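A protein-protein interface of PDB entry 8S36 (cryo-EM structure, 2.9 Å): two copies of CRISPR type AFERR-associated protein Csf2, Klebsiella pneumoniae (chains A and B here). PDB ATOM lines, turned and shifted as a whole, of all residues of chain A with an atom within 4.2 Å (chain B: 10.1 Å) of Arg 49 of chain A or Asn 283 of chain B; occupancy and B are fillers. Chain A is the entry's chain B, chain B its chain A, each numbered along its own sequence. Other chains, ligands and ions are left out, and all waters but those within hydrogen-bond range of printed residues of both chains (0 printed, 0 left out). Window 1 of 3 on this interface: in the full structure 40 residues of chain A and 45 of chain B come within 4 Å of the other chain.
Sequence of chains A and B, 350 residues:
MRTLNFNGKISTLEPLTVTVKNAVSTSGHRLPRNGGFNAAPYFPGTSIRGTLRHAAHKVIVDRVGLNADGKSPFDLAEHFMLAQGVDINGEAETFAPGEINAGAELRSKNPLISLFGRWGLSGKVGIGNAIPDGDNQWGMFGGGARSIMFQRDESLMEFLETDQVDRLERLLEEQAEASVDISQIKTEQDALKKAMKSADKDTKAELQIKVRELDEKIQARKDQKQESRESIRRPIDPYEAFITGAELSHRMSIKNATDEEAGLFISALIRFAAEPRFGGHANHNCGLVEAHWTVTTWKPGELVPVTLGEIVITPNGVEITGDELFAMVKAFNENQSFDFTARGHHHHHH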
ATOM      1  N   GLY A  45       3.144  14.018  -1.119  1.00  0.00           N
ATOM      2  CA  GLY A  45       3.966  15.212  -1.128  1.00  0.00           C
ATOM      3  C   GLY A  45       4.443  15.622   0.248  1.00  0.00           C
ATOM      4  O   GLY A  45       5.411  16.380   0.355  1.00  0.00           O
ATOM      5  N   THR A  46       3.814  15.105   1.304  1.00  0.00           N
ATOM      6  CA  THR A  46       4.237  15.434   2.660  1.00  0.00           C
ATOM      7  C   THR A  46       5.601  14.828   2.960  1.00  0.00           C
ATOM      8  O   THR A  46       6.483  15.500   3.504  1.00  0.00           O
ATOM      9  CB  THR A  46       3.202  14.950   3.675  1.00  0.00           C
ATOM     10  OG1 THR A  46       2.789  13.618   3.349  1.00  0.00           O
ATOM     11  CG2 THR A  46       1.990  15.862   3.682  1.00  0.00           C
ATOM     12  N   SER A  47       5.789  13.553   2.619  1.00  0.00           N
ATOM     13  CA  SER A  47       7.068  12.901   2.872  1.00  0.00           C
ATOM     14  C   SER A  47       8.183  13.544   2.058  1.00  0.00           C
ATOM     15  O   SER A  47       9.276  13.797   2.580  1.00  0.00           O
ATOM     16  CB  SER A  47       6.965  11.409   2.561  1.00  0.00           C
ATOM     17  OG  SER A  47       8.099  10.710   3.041  1.00  0.00           O
ATOM     18  N   ILE A  48       7.929  13.816   0.776  1.00  0.00           N
ATOM     19  CA  ILE A  48       8.949  14.458  -0.049  1.00  0.00           C
ATOM     20  C   ILE A  48       9.270  15.838   0.505  1.00  0.00           C
ATOM     21  O   ILE A  48      10.438  16.241   0.575  1.00  0.00           O
ATOM     22  CB  ILE A  48       8.498  14.547  -1.522  1.00  0.00           C
ATOM     23  CG1 ILE A  48       8.003  13.198  -2.052  1.00  0.00           C
ATOM     24  CG2 ILE A  48       9.647  15.046  -2.397  1.00  0.00           C
ATOM     25  CD1 ILE A  48       7.443  13.273  -3.462  1.00  0.00           C
ATOM     26  N   ARG A  49       8.239  16.588   0.899  1.00  0.00           N
ATOM     27  CA  ARG A  49       8.465  17.933   1.408  1.00  0.00           C
ATOM     28  C   ARG A  49       9.254  17.904   2.706  1.00  0.00           C
ATOM     29  O   ARG A  49      10.132  18.742   2.922  1.00  0.00           O
ATOM     30  CB  ARG A  49       7.127  18.635   1.624  1.00  0.00           C
ATOM     31  CG  ARG A  49       7.232  20.134   1.784  1.00  0.00           C
ATOM     32  CD  ARG A  49       5.851  20.749   1.907  1.00  0.00           C
ATOM     33  NE  ARG A  49       5.802  22.154   1.515  1.00  0.00           N
ATOM     34  CZ  ARG A  49       6.434  23.144   2.133  1.00  0.00           C
ATOM     35  NH1 ARG A  49       7.249  22.924   3.151  1.00  0.00           N
ATOM     36  NH2 ARG A  49       6.243  24.392   1.717  1.00  0.00           N
ATOM     37  N   GLY A  50       8.965  16.941   3.580  1.00  0.00           N
ATOM     38  CA  GLY A  50       9.723  16.832   4.813  1.00  0.00           C
ATOM     39  C   GLY A  50      11.167  16.434   4.573  1.00  0.00           C
ATOM     40  O   GLY A  50      12.081  16.970   5.205  1.00  0.00           O
ATOM     41  N   THR A  51      11.393  15.496   3.651  1.00  0.00           N
ATOM     42  CA  THR A  51      12.758  15.113   3.316  1.00  0.00           C
ATOM     43  C   THR A  51      13.533  16.302   2.766  1.00  0.00           C
ATOM     44  O   THR A  51      14.676  16.549   3.166  1.00  0.00           O
ATOM     45  CB  THR A  51      12.750  13.966   2.308  1.00  0.00           C
ATOM     46  OG1 THR A  51      12.114  12.821   2.888  1.00  0.00           O
ATOM     47  CG2 THR A  51      14.168  13.603   1.896  1.00  0.00           C
ATOM     48  N   LEU A  52      12.916  17.064   1.863  1.00  0.00           N
ATOM     49  CA  LEU A  52      13.597  18.218   1.290  1.00  0.00           C
ATOM     50  C   LEU A  52      13.797  19.316   2.324  1.00  0.00           C
ATOM     51  O   LEU A  52      14.816  20.011   2.294  1.00  0.00           O
ATOM     52  CB  LEU A  52      12.813  18.749   0.092  1.00  0.00           C
ATOM     53  CG  LEU A  52      13.266  18.211  -1.268  1.00  0.00           C
ATOM     54  CD1 LEU A  52      13.348  16.693  -1.253  1.00  0.00           C
ATOM     55  CD2 LEU A  52      12.331  18.682  -2.365  1.00  0.00           C
ATOM     56  N   ARG A  53      12.850  19.487   3.247  1.00  0.00           N
ATOM     57  CA  ARG A  53      13.013  20.488   4.292  1.00  0.00           C
ATOM     58  C   ARG A  53      14.149  20.117   5.233  1.00  0.00           C
ATOM     59  O   ARG A  53      14.919  20.987   5.656  1.00  0.00           O
ATOM     60  CB  ARG A  53      11.706  20.647   5.066  1.00  0.00           C
ATOM     61  CG  ARG A  53      11.723  21.777   6.077  1.00  0.00           C
ATOM     62  CD  ARG A  53      10.323  22.119   6.552  1.00  0.00           C
ATOM     63  NE  ARG A  53      10.313  23.327   7.371  1.00  0.00           N
ATOM     64  CZ  ARG A  53       9.272  24.139   7.515  1.00  0.00           C
ATOM     65  NH1 ARG A  53       8.116  23.902   6.916  1.00  0.00           N
ATOM     66  NH2 ARG A  53       9.397  25.217   8.282  1.00  0.00           N
ATOM     67  N   LEU A 115      11.063  29.570   2.164  1.00  0.00           N
ATOM     68  CA  LEU A 115      10.814  28.478   1.232  1.00  0.00           C
ATOM     69  C   LEU A 115       9.780  27.512   1.794  1.00  0.00           C
ATOM     70  O   LEU A 115       8.718  27.301   1.198  1.00  0.00           O
ATOM     71  CB  LEU A 115      12.115  27.728   0.948  1.00  0.00           C
ATOM     72  CG  LEU A 115      13.141  28.314  -0.015  1.00  0.00           C
ATOM     73  CD1 LEU A 115      14.397  27.474   0.082  1.00  0.00           C
ATOM     74  CD2 LEU A 115      12.628  28.339  -1.442  1.00  0.00           C
ATOM     75  N   PHE A 116      10.064  26.929   2.956  1.00  0.00           N
ATOM     76  CA  PHE A 116       9.231  25.878   3.519  1.00  0.00           C
ATOM     77  C   PHE A 116       8.200  26.393   4.513  1.00  0.00           C
ATOM     78  O   PHE A 116       7.497  25.584   5.127  1.00  0.00           O
ATOM     79  CB  PHE A 116      10.112  24.822   4.188  1.00  0.00           C
ATOM     80  CG  PHE A 116      10.994  24.081   3.227  1.00  0.00           C
ATOM     81  CD1 PHE A 116      10.542  22.938   2.592  1.00  0.00           C
ATOM     82  CD2 PHE A 116      12.272  24.532   2.951  1.00  0.00           C
ATOM     83  CE1 PHE A 116      11.350  22.255   1.707  1.00  0.00           C
ATOM     84  CE2 PHE A 116      13.084  23.854   2.066  1.00  0.00           C
ATOM     85  CZ  PHE A 116      12.623  22.714   1.442  1.00  0.00           C
ATOM     86  N   VAL A 125       7.679  27.237  -1.148  1.00  0.00           N
ATOM     87  CA  VAL A 125       7.832  25.910  -1.731  1.00  0.00           C
ATOM     88  C   VAL A 125       6.537  25.128  -1.556  1.00  0.00           C
ATOM     89  O   VAL A 125       5.990  25.043  -0.452  1.00  0.00           O
ATOM     90  CB  VAL A 125       9.016  25.171  -1.091  1.00  0.00           C
ATOM     91  CG1 VAL A 125       8.977  23.694  -1.438  1.00  0.00           C
ATOM     92  CG2 VAL A 125      10.323  25.790  -1.540  1.00  0.00           C
ATOM     93  N   GLY A 126       6.044  24.567  -2.653  1.00  0.00           N
ATOM     94  CA  GLY A 126       5.000  23.568  -2.643  1.00  0.00           C
ATOM     95  C   GLY A 126       5.499  22.301  -3.304  1.00  0.00           C
ATOM     96  O   GLY A 126       5.789  22.302  -4.504  1.00  0.00           O
ATOM     97  N   ILE A 127       5.611  21.222  -2.539  1.00  0.00           N
ATOM     98  CA  ILE A 127       6.141  19.953  -3.026  1.00  0.00           C
ATOM     99  C   ILE A 127       4.960  19.035  -3.303  1.00  0.00           C
ATOM    100  O   ILE A 127       4.320  18.532  -2.374  1.00  0.00           O
ATOM    101  CB  ILE A 127       7.114  19.320  -2.023  1.00  0.00           C
ATOM    102  CG1 ILE A 127       8.258  20.283  -1.690  1.00  0.00           C
ATOM    103  CG2 ILE A 127       7.658  18.012  -2.568  1.00  0.00           C
ATOM    104  CD1 ILE A 127       9.238  20.515  -2.817  1.00  0.00           C
ATOM    105  N   GLU B  14      -1.969  18.872  -9.422  1.00  0.00           N
ATOM    106  CA  GLU B  14      -1.756  18.429  -8.057  1.00  0.00           C
ATOM    107  C   GLU B  14      -3.049  18.607  -7.275  1.00  0.00           C
ATOM    108  O   GLU B  14      -3.816  19.532  -7.557  1.00  0.00           O
ATOM    109  CB  GLU B  14      -0.621  19.214  -7.380  1.00  0.00           C
ATOM    110  CG  GLU B  14       0.793  18.746  -7.736  1.00  0.00           C
ATOM    111  CD  GLU B  14       0.994  17.250  -7.572  1.00  0.00           C
ATOM    112  OE1 GLU B  14       0.773  16.507  -8.551  1.00  0.00           O
ATOM    113  OE2 GLU B  14       1.353  16.810  -6.461  1.00  0.00           O
ATOM    114  N   PRO B  15      -3.319  17.729  -6.300  1.00  0.00           N
ATOM    115  CA  PRO B  15      -4.660  17.657  -5.698  1.00  0.00           C
ATOM    116  C   PRO B  15      -5.253  19.019  -5.358  1.00  0.00           C
ATOM    117  O   PRO B  15      -4.558  19.930  -4.906  1.00  0.00           O
ATOM    118  CB  PRO B  15      -4.439  16.815  -4.433  1.00  0.00           C
ATOM    119  CG  PRO B  15      -2.963  16.655  -4.287  1.00  0.00           C
ATOM    120  CD  PRO B  15      -2.380  16.809  -5.642  1.00  0.00           C
ATOM    121  N   THR B  17      -7.752  21.092  -3.163  1.00  0.00           N
ATOM    122  CA  THR B  17      -8.419  21.078  -1.867  1.00  0.00           C
ATOM    123  C   THR B  17      -8.862  22.483  -1.485  1.00  0.00           C
ATOM    124  O   THR B  17      -8.320  23.482  -1.964  1.00  0.00           O
ATOM    125  CB  THR B  17      -7.505  20.520  -0.770  1.00  0.00           C
ATOM    126  OG1 THR B  17      -8.270  20.284   0.418  1.00  0.00           O
ATOM    127  CG2 THR B  17      -6.383  21.495  -0.461  1.00  0.00           C
ATOM    128  N   THR B  19     -10.696  24.484   2.218  1.00  0.00           N
ATOM    129  CA  THR B  19     -11.235  24.441   3.571  1.00  0.00           C
ATOM    130  C   THR B  19     -12.470  25.330   3.633  1.00  0.00           C
ATOM    131  O   THR B  19     -12.394  26.524   3.329  1.00  0.00           O
ATOM    132  CB  THR B  19     -10.195  24.900   4.593  1.00  0.00           C
ATOM    133  OG1 THR B  19      -8.922  24.324   4.275  1.00  0.00           O
ATOM    134  CG2 THR B  19     -10.595  24.484   6.000  1.00  0.00           C
ATOM    135  N   PHE B 141      -5.961  13.284   1.182  1.00  0.00           N
ATOM    136  CA  PHE B 141      -4.558  13.513   0.869  1.00  0.00           C
ATOM    137  C   PHE B 141      -3.865  14.201   2.043  1.00  0.00           C
ATOM    138  O   PHE B 141      -4.479  14.509   3.074  1.00  0.00           O
ATOM    139  CB  PHE B 141      -4.422  14.351  -0.405  1.00  0.00           C
ATOM    140  CG  PHE B 141      -4.916  13.662  -1.638  1.00  0.00           C
ATOM    141  CD1 PHE B 141      -6.256  13.686  -1.967  1.00  0.00           C
ATOM    142  CD2 PHE B 141      -4.038  13.003  -2.478  1.00  0.00           C
ATOM    143  CE1 PHE B 141      -6.715  13.058  -3.102  1.00  0.00           C
ATOM    144  CE2 PHE B 141      -4.491  12.372  -3.615  1.00  0.00           C
ATOM    145  CZ  PHE B 141      -5.832  12.400  -3.928  1.00  0.00           C
ATOM    146  N   GLY B 142      -2.588  14.505   1.839  1.00  0.00           N
ATOM    147  CA  GLY B 142      -1.762  15.079   2.889  1.00  0.00           C
ATOM    148  C   GLY B 142      -1.722  14.201   4.121  1.00  0.00           C
ATOM    149  O   GLY B 142      -1.352  13.022   4.065  1.00  0.00           O
ATOM    150  N   GLY B 143      -2.115  14.777   5.252  1.00  0.00           N
ATOM    151  CA  GLY B 143      -1.979  14.091   6.524  1.00  0.00           C
ATOM    152  C   GLY B 143      -0.542  13.693   6.793  1.00  0.00           C
ATOM    153  O   GLY B 143       0.402  14.434   6.497  1.00  0.00           O
ATOM    154  N   ALA B 145       2.385  12.770   9.513  1.00  0.00           N
ATOM    155  CA  ALA B 145       2.738  13.069  10.895  1.00  0.00           C
ATOM    156  C   ALA B 145       3.937  14.004  10.903  1.00  0.00           C
ATOM    157  O   ALA B 145       4.707  14.060   9.939  1.00  0.00           O
ATOM    158  CB  ALA B 145       3.051  11.794  11.684  1.00  0.00           C
ATOM    159  N   SER B 147       6.957  13.914  12.465  1.00  0.00           N
ATOM    160  CA  SER B 147       7.970  13.135  13.165  1.00  0.00           C
ATOM    161  C   SER B 147       8.996  14.044  13.834  1.00  0.00           C
ATOM    162  O   SER B 147       9.426  15.051  13.265  1.00  0.00           O
ATOM    163  CB  SER B 147       8.669  12.186  12.193  1.00  0.00           C
ATOM    164  OG  SER B 147       9.390  12.905  11.209  1.00  0.00           O
ATOM    165  N   ARG B 152      14.164  10.545  14.341  1.00  0.00           N
ATOM    166  CA  ARG B 152      14.231   9.923  13.022  1.00  0.00           C
ATOM    167  C   ARG B 152      15.677   9.778  12.556  1.00  0.00           C
ATOM    168  O   ARG B 152      16.136   8.670  12.264  1.00  0.00           O
ATOM    169  CB  ARG B 152      13.420  10.754  12.020  1.00  0.00           C
ATOM    170  CG  ARG B 152      13.407  10.222  10.590  1.00  0.00           C
ATOM    171  CD  ARG B 152      12.579   8.958  10.470  1.00  0.00           C
ATOM    172  NE  ARG B 152      11.158   9.232  10.646  1.00  0.00           N
ATOM    173  CZ  ARG B 152      10.379   9.784   9.725  1.00  0.00           C
ATOM    174  NH1 ARG B 152      10.847  10.134   8.538  1.00  0.00           N
ATOM    175  NH2 ARG B 152       9.095   9.992  10.004  1.00  0.00           N
ATOM    176  N   ILE B 236      -0.865  14.374  11.460  1.00  0.00           N
ATOM    177  CA  ILE B 236      -1.538  15.431  10.713  1.00  0.00           C
ATOM    178  C   ILE B 236      -2.819  14.871  10.117  1.00  0.00           C
ATOM    179  O   ILE B 236      -2.806  13.833   9.444  1.00  0.00           O
ATOM    180  CB  ILE B 236      -0.617  15.992   9.619  1.00  0.00           C
ATOM    181  CG1 ILE B 236       0.773  16.294  10.188  1.00  0.00           C
ATOM    182  CG2 ILE B 236      -1.235  17.231   8.977  1.00  0.00           C
ATOM    183  CD1 ILE B 236       0.767  17.091  11.481  1.00  0.00           C
ATOM    184  N   ASP B 237      -3.930  15.545  10.374  1.00  0.00           N
ATOM    185  CA  ASP B 237      -5.198  15.106   9.817  1.00  0.00           C
ATOM    186  C   ASP B 237      -5.168  15.275   8.300  1.00  0.00           C
ATOM    187  O   ASP B 237      -4.762  16.336   7.813  1.00  0.00           O
ATOM    188  CB  ASP B 237      -6.349  15.911  10.415  1.00  0.00           C
ATOM    189  CG  ASP B 237      -6.770  15.404  11.781  1.00  0.00           C
ATOM    190  OD1 ASP B 237      -6.839  14.171  11.968  1.00  0.00           O
ATOM    191  OD2 ASP B 237      -7.030  16.241  12.671  1.00  0.00           O
ATOM    192  N   TYR B 239      -6.476  16.121   4.553  1.00  0.00           N
ATOM    193  CA  TYR B 239      -7.480  16.996   3.969  1.00  0.00           C
ATOM    194  C   TYR B 239      -8.048  16.341   2.720  1.00  0.00           C
ATOM    195  O   TYR B 239      -7.350  15.614   2.015  1.00  0.00           O
ATOM    196  CB  TYR B 239      -6.893  18.363   3.610  1.00  0.00           C
ATOM    197  CG  TYR B 239      -5.643  18.281   2.769  1.00  0.00           C
ATOM    198  CD1 TYR B 239      -5.712  18.072   1.399  1.00  0.00           C
ATOM    199  CD2 TYR B 239      -4.392  18.401   3.349  1.00  0.00           C
ATOM    200  CE1 TYR B 239      -4.573  17.988   0.634  1.00  0.00           C
ATOM    201  CE2 TYR B 239      -3.251  18.327   2.593  1.00  0.00           C
ATOM    202  CZ  TYR B 239      -3.344  18.114   1.237  1.00  0.00           C
ATOM    203  OH  TYR B 239      -2.195  18.036   0.483  1.00  0.00           O
ATOM    204  N   GLU B 275       0.778  31.053 -12.108  1.00  0.00           N
ATOM    205  CA  GLU B 275       0.645  30.263 -10.885  1.00  0.00           C
ATOM    206  C   GLU B 275      -0.771  29.704 -10.863  1.00  0.00           C
ATOM    207  O   GLU B 275      -1.636  30.205 -10.131  1.00  0.00           O
ATOM    208  CB  GLU B 275       0.931  31.111  -9.644  1.00  0.00           C
ATOM    209  CG  GLU B 275       0.894  30.342  -8.325  1.00  0.00           C
ATOM    210  CD  GLU B 275       2.184  29.596  -8.037  1.00  0.00           C
ATOM    211  OE1 GLU B 275       3.266  30.108  -8.391  1.00  0.00           O
ATOM    212  OE2 GLU B 275       2.114  28.494  -7.454  1.00  0.00           O
ATOM    213  N   ARG B 277      -2.926  28.104  -9.340  1.00  0.00           N
ATOM    214  CA  ARG B 277      -3.180  27.488  -8.042  1.00  0.00           C
ATOM    215  C   ARG B 277      -4.580  27.855  -7.571  1.00  0.00           C
ATOM    216  O   ARG B 277      -4.922  29.039  -7.487  1.00  0.00           O
ATOM    217  CB  ARG B 277      -2.139  27.934  -7.018  1.00  0.00           C
ATOM    218  CG  ARG B 277      -1.853  26.899  -5.941  1.00  0.00           C
ATOM    219  CD  ARG B 277      -0.564  27.209  -5.200  1.00  0.00           C
ATOM    220  NE  ARG B 277       0.608  27.038  -6.049  1.00  0.00           N
ATOM    221  CZ  ARG B 277       1.091  25.866  -6.440  1.00  0.00           C
ATOM    222  NH1 ARG B 277       0.530  24.726  -6.072  1.00  0.00           N
ATOM    223  NH2 ARG B 277       2.167  25.838  -7.221  1.00  0.00           N
ATOM    224  N   PHE B 278      -5.381  26.836  -7.269  1.00  0.00           N
ATOM    225  CA  PHE B 278      -6.698  26.994  -6.672  1.00  0.00           C
ATOM    226  C   PHE B 278      -6.695  26.377  -5.282  1.00  0.00           C
ATOM    227  O   PHE B 278      -6.156  25.285  -5.078  1.00  0.00           O
ATOM    228  CB  PHE B 278      -7.789  26.327  -7.522  1.00  0.00           C
ATOM    229  CG  PHE B 278      -8.182  27.102  -8.752  1.00  0.00           C
ATOM    230  CD1 PHE B 278      -8.370  28.474  -8.710  1.00  0.00           C
ATOM    231  CD2 PHE B 278      -8.387  26.445  -9.953  1.00  0.00           C
ATOM    232  CE1 PHE B 278      -8.737  29.172  -9.840  1.00  0.00           C
ATOM    233  CE2 PHE B 278      -8.755  27.140 -11.086  1.00  0.00           C
ATOM    234  CZ  PHE B 278      -8.933  28.504 -11.028  1.00  0.00           C
ATOM    235  N   GLY B 279      -7.302  27.073  -4.332  1.00  0.00           N
ATOM    236  CA  GLY B 279      -7.422  26.534  -2.996  1.00  0.00           C
ATOM    237  C   GLY B 279      -6.107  26.540  -2.232  1.00  0.00           C
ATOM    238  O   GLY B 279      -5.117  27.164  -2.616  1.00  0.00           O
ATOM    239  N   GLY B 280      -6.122  25.812  -1.119  1.00  0.00           N
ATOM    240  CA  GLY B 280      -5.068  25.861  -0.133  1.00  0.00           C
ATOM    241  C   GLY B 280      -4.157  24.651  -0.159  1.00  0.00           C
ATOM    242  O   GLY B 280      -4.064  23.921  -1.151  1.00  0.00           O
ATOM    243  N   HIS B 281      -3.477  24.438   0.967  1.00  0.00           N
ATOM    244  CA  HIS B 281      -2.432  23.428   1.094  1.00  0.00           C
ATOM    245  C   HIS B 281      -1.408  23.552  -0.029  1.00  0.00           C
ATOM    246  O   HIS B 281      -0.981  22.563  -0.628  1.00  0.00           O
ATOM    247  CB  HIS B 281      -3.038  22.029   1.150  1.00  0.00           C
ATOM    248  CG  HIS B 281      -3.821  21.773   2.400  1.00  0.00           C
ATOM    249  ND1 HIS B 281      -5.199  21.747   2.425  1.00  0.00           N
ATOM    250  CD2 HIS B 281      -3.417  21.559   3.674  1.00  0.00           C
ATOM    251  CE1 HIS B 281      -5.610  21.514   3.658  1.00  0.00           C
ATOM    252  NE2 HIS B 281      -4.550  21.395   4.435  1.00  0.00           N
ATOM    253  N   ALA B 282      -0.992  24.790  -0.304  1.00  0.00           N
ATOM    254  CA  ALA B 282       0.058  25.030  -1.285  1.00  0.00           C
ATOM    255  C   ALA B 282       1.410  24.497  -0.833  1.00  0.00           C
ATOM    256  O   ALA B 282       2.338  24.444  -1.647  1.00  0.00           O
ATOM    257  CB  ALA B 282       0.168  26.525  -1.578  1.00  0.00           C
ATOM    258  N   ASN B 283       1.546  24.103   0.436  1.00  0.00           N
ATOM    259  CA  ASN B 283       2.775  23.455   0.880  1.00  0.00           C
ATOM    260  C   ASN B 283       2.985  22.140   0.145  1.00  0.00           C
ATOM    261  O   ASN B 283       4.118  21.779  -0.191  1.00  0.00           O
ATOM    262  CB  ASN B 283       2.733  23.225   2.389  1.00  0.00           C
ATOM    263  CG  ASN B 283       1.537  22.402   2.820  1.00  0.00           C
ATOM    264  OD1 ASN B 283       0.610  22.183   2.040  1.00  0.00           O
ATOM    265  ND2 ASN B 283       1.552  21.942   4.064  1.00  0.00           N
ATOM    266  N   HIS B 284       1.908  21.397  -0.086  1.00  0.00           N
ATOM    267  CA  HIS B 284       1.947  20.176  -0.873  1.00  0.00           C
ATOM    268  C   HIS B 284       1.672  20.430  -2.350  1.00  0.00           C
ATOM    269  O   HIS B 284       1.220  19.520  -3.054  1.00  0.00           O
ATOM    270  CB  HIS B 284       0.955  19.160  -0.307  1.00  0.00           C
ATOM    271  CG  HIS B 284       1.026  19.023   1.180  1.00  0.00           C
ATOM    272  ND1 HIS B 284      -0.066  18.694   1.950  1.00  0.00           N
ATOM    273  CD2 HIS B 284       2.060  19.176   2.042  1.00  0.00           C
ATOM    274  CE1 HIS B 284       0.289  18.649   3.222  1.00  0.00           C
ATOM    275  NE2 HIS B 284       1.575  18.939   3.305  1.00  0.00           N
ATOM    276  N   ASN B 285       1.908  21.653  -2.827  1.00  0.00           N
ATOM    277  CA  ASN B 285       1.675  22.030  -4.219  1.00  0.00           C
ATOM    278  C   ASN B 285       0.225  21.842  -4.642  1.00  0.00           C
ATOM    279  O   ASN B 285      -0.075  21.800  -5.838  1.00  0.00           O
ATOM    280  CB  ASN B 285       2.593  21.246  -5.163  1.00  0.00           C
ATOM    281  CG  ASN B 285       2.808  21.952  -6.488  1.00  0.00           C
ATOM    282  OD1 ASN B 285       2.311  23.056  -6.706  1.00  0.00           O
ATOM    283  ND2 ASN B 285       3.550  21.312  -7.382  1.00  0.00           N
ATOM    284  N   CYS B 286      -0.689  21.723  -3.683  1.00  0.00           N
ATOM    285  CA  CYS B 286      -2.088  21.511  -4.017  1.00  0.00           C
ATOM    286  C   CYS B 286      -2.645  22.718  -4.754  1.00  0.00           C
ATOM    287  O   CYS B 286      -2.295  23.865  -4.460  1.00  0.00           O
ATOM    288  CB  CYS B 286      -2.904  21.262  -2.754  1.00  0.00           C
ATOM    289  SG  CYS B 286      -2.480  19.754  -1.884  1.00  0.00           S
ATOM    290  N   GLY B 287      -3.513  22.452  -5.723  1.00  0.00           N
ATOM    291  CA  GLY B 287      -4.175  23.487  -6.478  1.00  0.00           C
ATOM    292  C   GLY B 287      -3.622  23.719  -7.865  1.00  0.00           C
ATOM    293  O   GLY B 287      -4.255  24.438  -8.647  1.00  0.00           O
ATOM    294  N   LEU B 288      -2.470  23.145  -8.198  1.00  0.00           N
ATOM    295  CA  LEU B 288      -1.954  23.291  -9.550  1.00  0.00           C
ATOM    296  C   LEU B 288      -2.923  22.645 -10.529  1.00  0.00           C
ATOM    297  O   LEU B 288      -3.208  21.448 -10.434  1.00  0.00           O
ATOM    298  CB  LEU B 288      -0.568  22.654  -9.656  1.00  0.00           C
ATOM    299  CG  LEU B 288       0.410  23.080 -10.762  1.00  0.00           C
ATOM    300  CD1 LEU B 288       0.248  24.531 -11.203  1.00  0.00           C
ATOM    301  CD2 LEU B 288       1.841  22.831 -10.305  1.00  0.00           C
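O of Asn 283 of chain B is in hydrogen-bond range of NE of Arg 49 of chain A, 2.4 Å away. The backbone carbonyl oxygen (O) of Ile 127 of chain A lies close to the backbone carbonyl oxygen (O) of His 284 of chain B (3.3 Å). N of Ile 127 of chain A is in hydrogen-bond range of O of Asn 283 of chain B, at 2.8 Å.
The side-chain hydroxyl of Tyr 239 of chain B lies within hydrogen-bond range of a ring nitrogen (ND1) of His 284 of chain B, at 2.7 Å. The backbone carbonyl oxygen (O) of His 281 of chain B sits close to the side-chain amide oxygen (OD1) of Asn 283 of chain B (3.1 Å). The side-chain amide nitrogen (ND2) of Asn 283 of chain B is in hydrogen-bond range of a ring nitrogen (NE2) of His 284 of chain B, at 3.1 Å. The side-chain amide oxygen (OD1) of Asn 285 of chain B is in hydrogen-bond range of the guanidinium group (NH1) of Arg 277 of chain B (2.5 Å). NH1 of Arg 49 of chain A is in hydrogen-bond range of O of Phe 116 of chain A (3.3 Å).
Among the printed residues, pairs that only touch across the chains: Thr 46 of chain A with Gly 142 of chain B (3.9 Å), Thr 46 of chain A with Gly 143 of chain B (3.5 Å), Thr 46 of chain A with His 284 of chain B (3.1 Å), Val 125 of chain A with Ala 282 of chain B (3.9 Å), Val 125 of chain A with Asn 283 of chain B (3.8 Å), Gly 126 of chain A with Ala 282 of chain B (3.0 Å), Gly 126 of chain A with Asn 283 of chain B (3.2 Å), Gly 126 of chain A with Asn 285 of chain B (3.4 Å) and Ile 127 of chain A with Asn 285 of chain B (3.7 Å).
Of the printed residues of chain B, Thr 46 of chain A touches Gly 142, Gly 143 and His 284. No residue of chain B comes within 4 Å of Ile 48 of chain A. Arg 49 of chain A touches just one residue of chain B: Asn 283 (2.4 Å). No residue of chain B comes within 4 Å of Leu 52 of chain A. Arg 53 of chain A touches none of the printed residues of chain B. No residue of chain B comes within 4 Å of Phe 116 of chain A. Val 125 of chain A touches two residues of chain B. Ile 127 of chain A touches just these residues of chain B: Asn 283, His 284 and Asn 285. Phe 278 of chain B touches none of the printed residues of chain A. Gly 280 of chain B touches none of the printed residues of chain A. Printed residues of chain A within 4 Å of Ala 282 of chain B: Val 125 and Gly 126. Printed residues of chain A within 4 Å of His 284 of chain B: Thr 46 (3.1 Å) and Ile 127 (3.3 Å).
Of the 26 printed residues of chain B, 6 touch a printed residue of chain A. Hydrophobic or aromatic side chains of chain B that line the printed part of chain A: His 284. Among the printed residues, 12 pairs touch across the chains. Among the printed residues, no Asp or Glu carboxylate lies within 4 Å of a Lys or Arg side-chain nitrogen of the other chain.
No position is printed for both chains. Of the 12 pairs that touch across the chains among the printed residues, none has its exchanged pair printed and touching as well.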
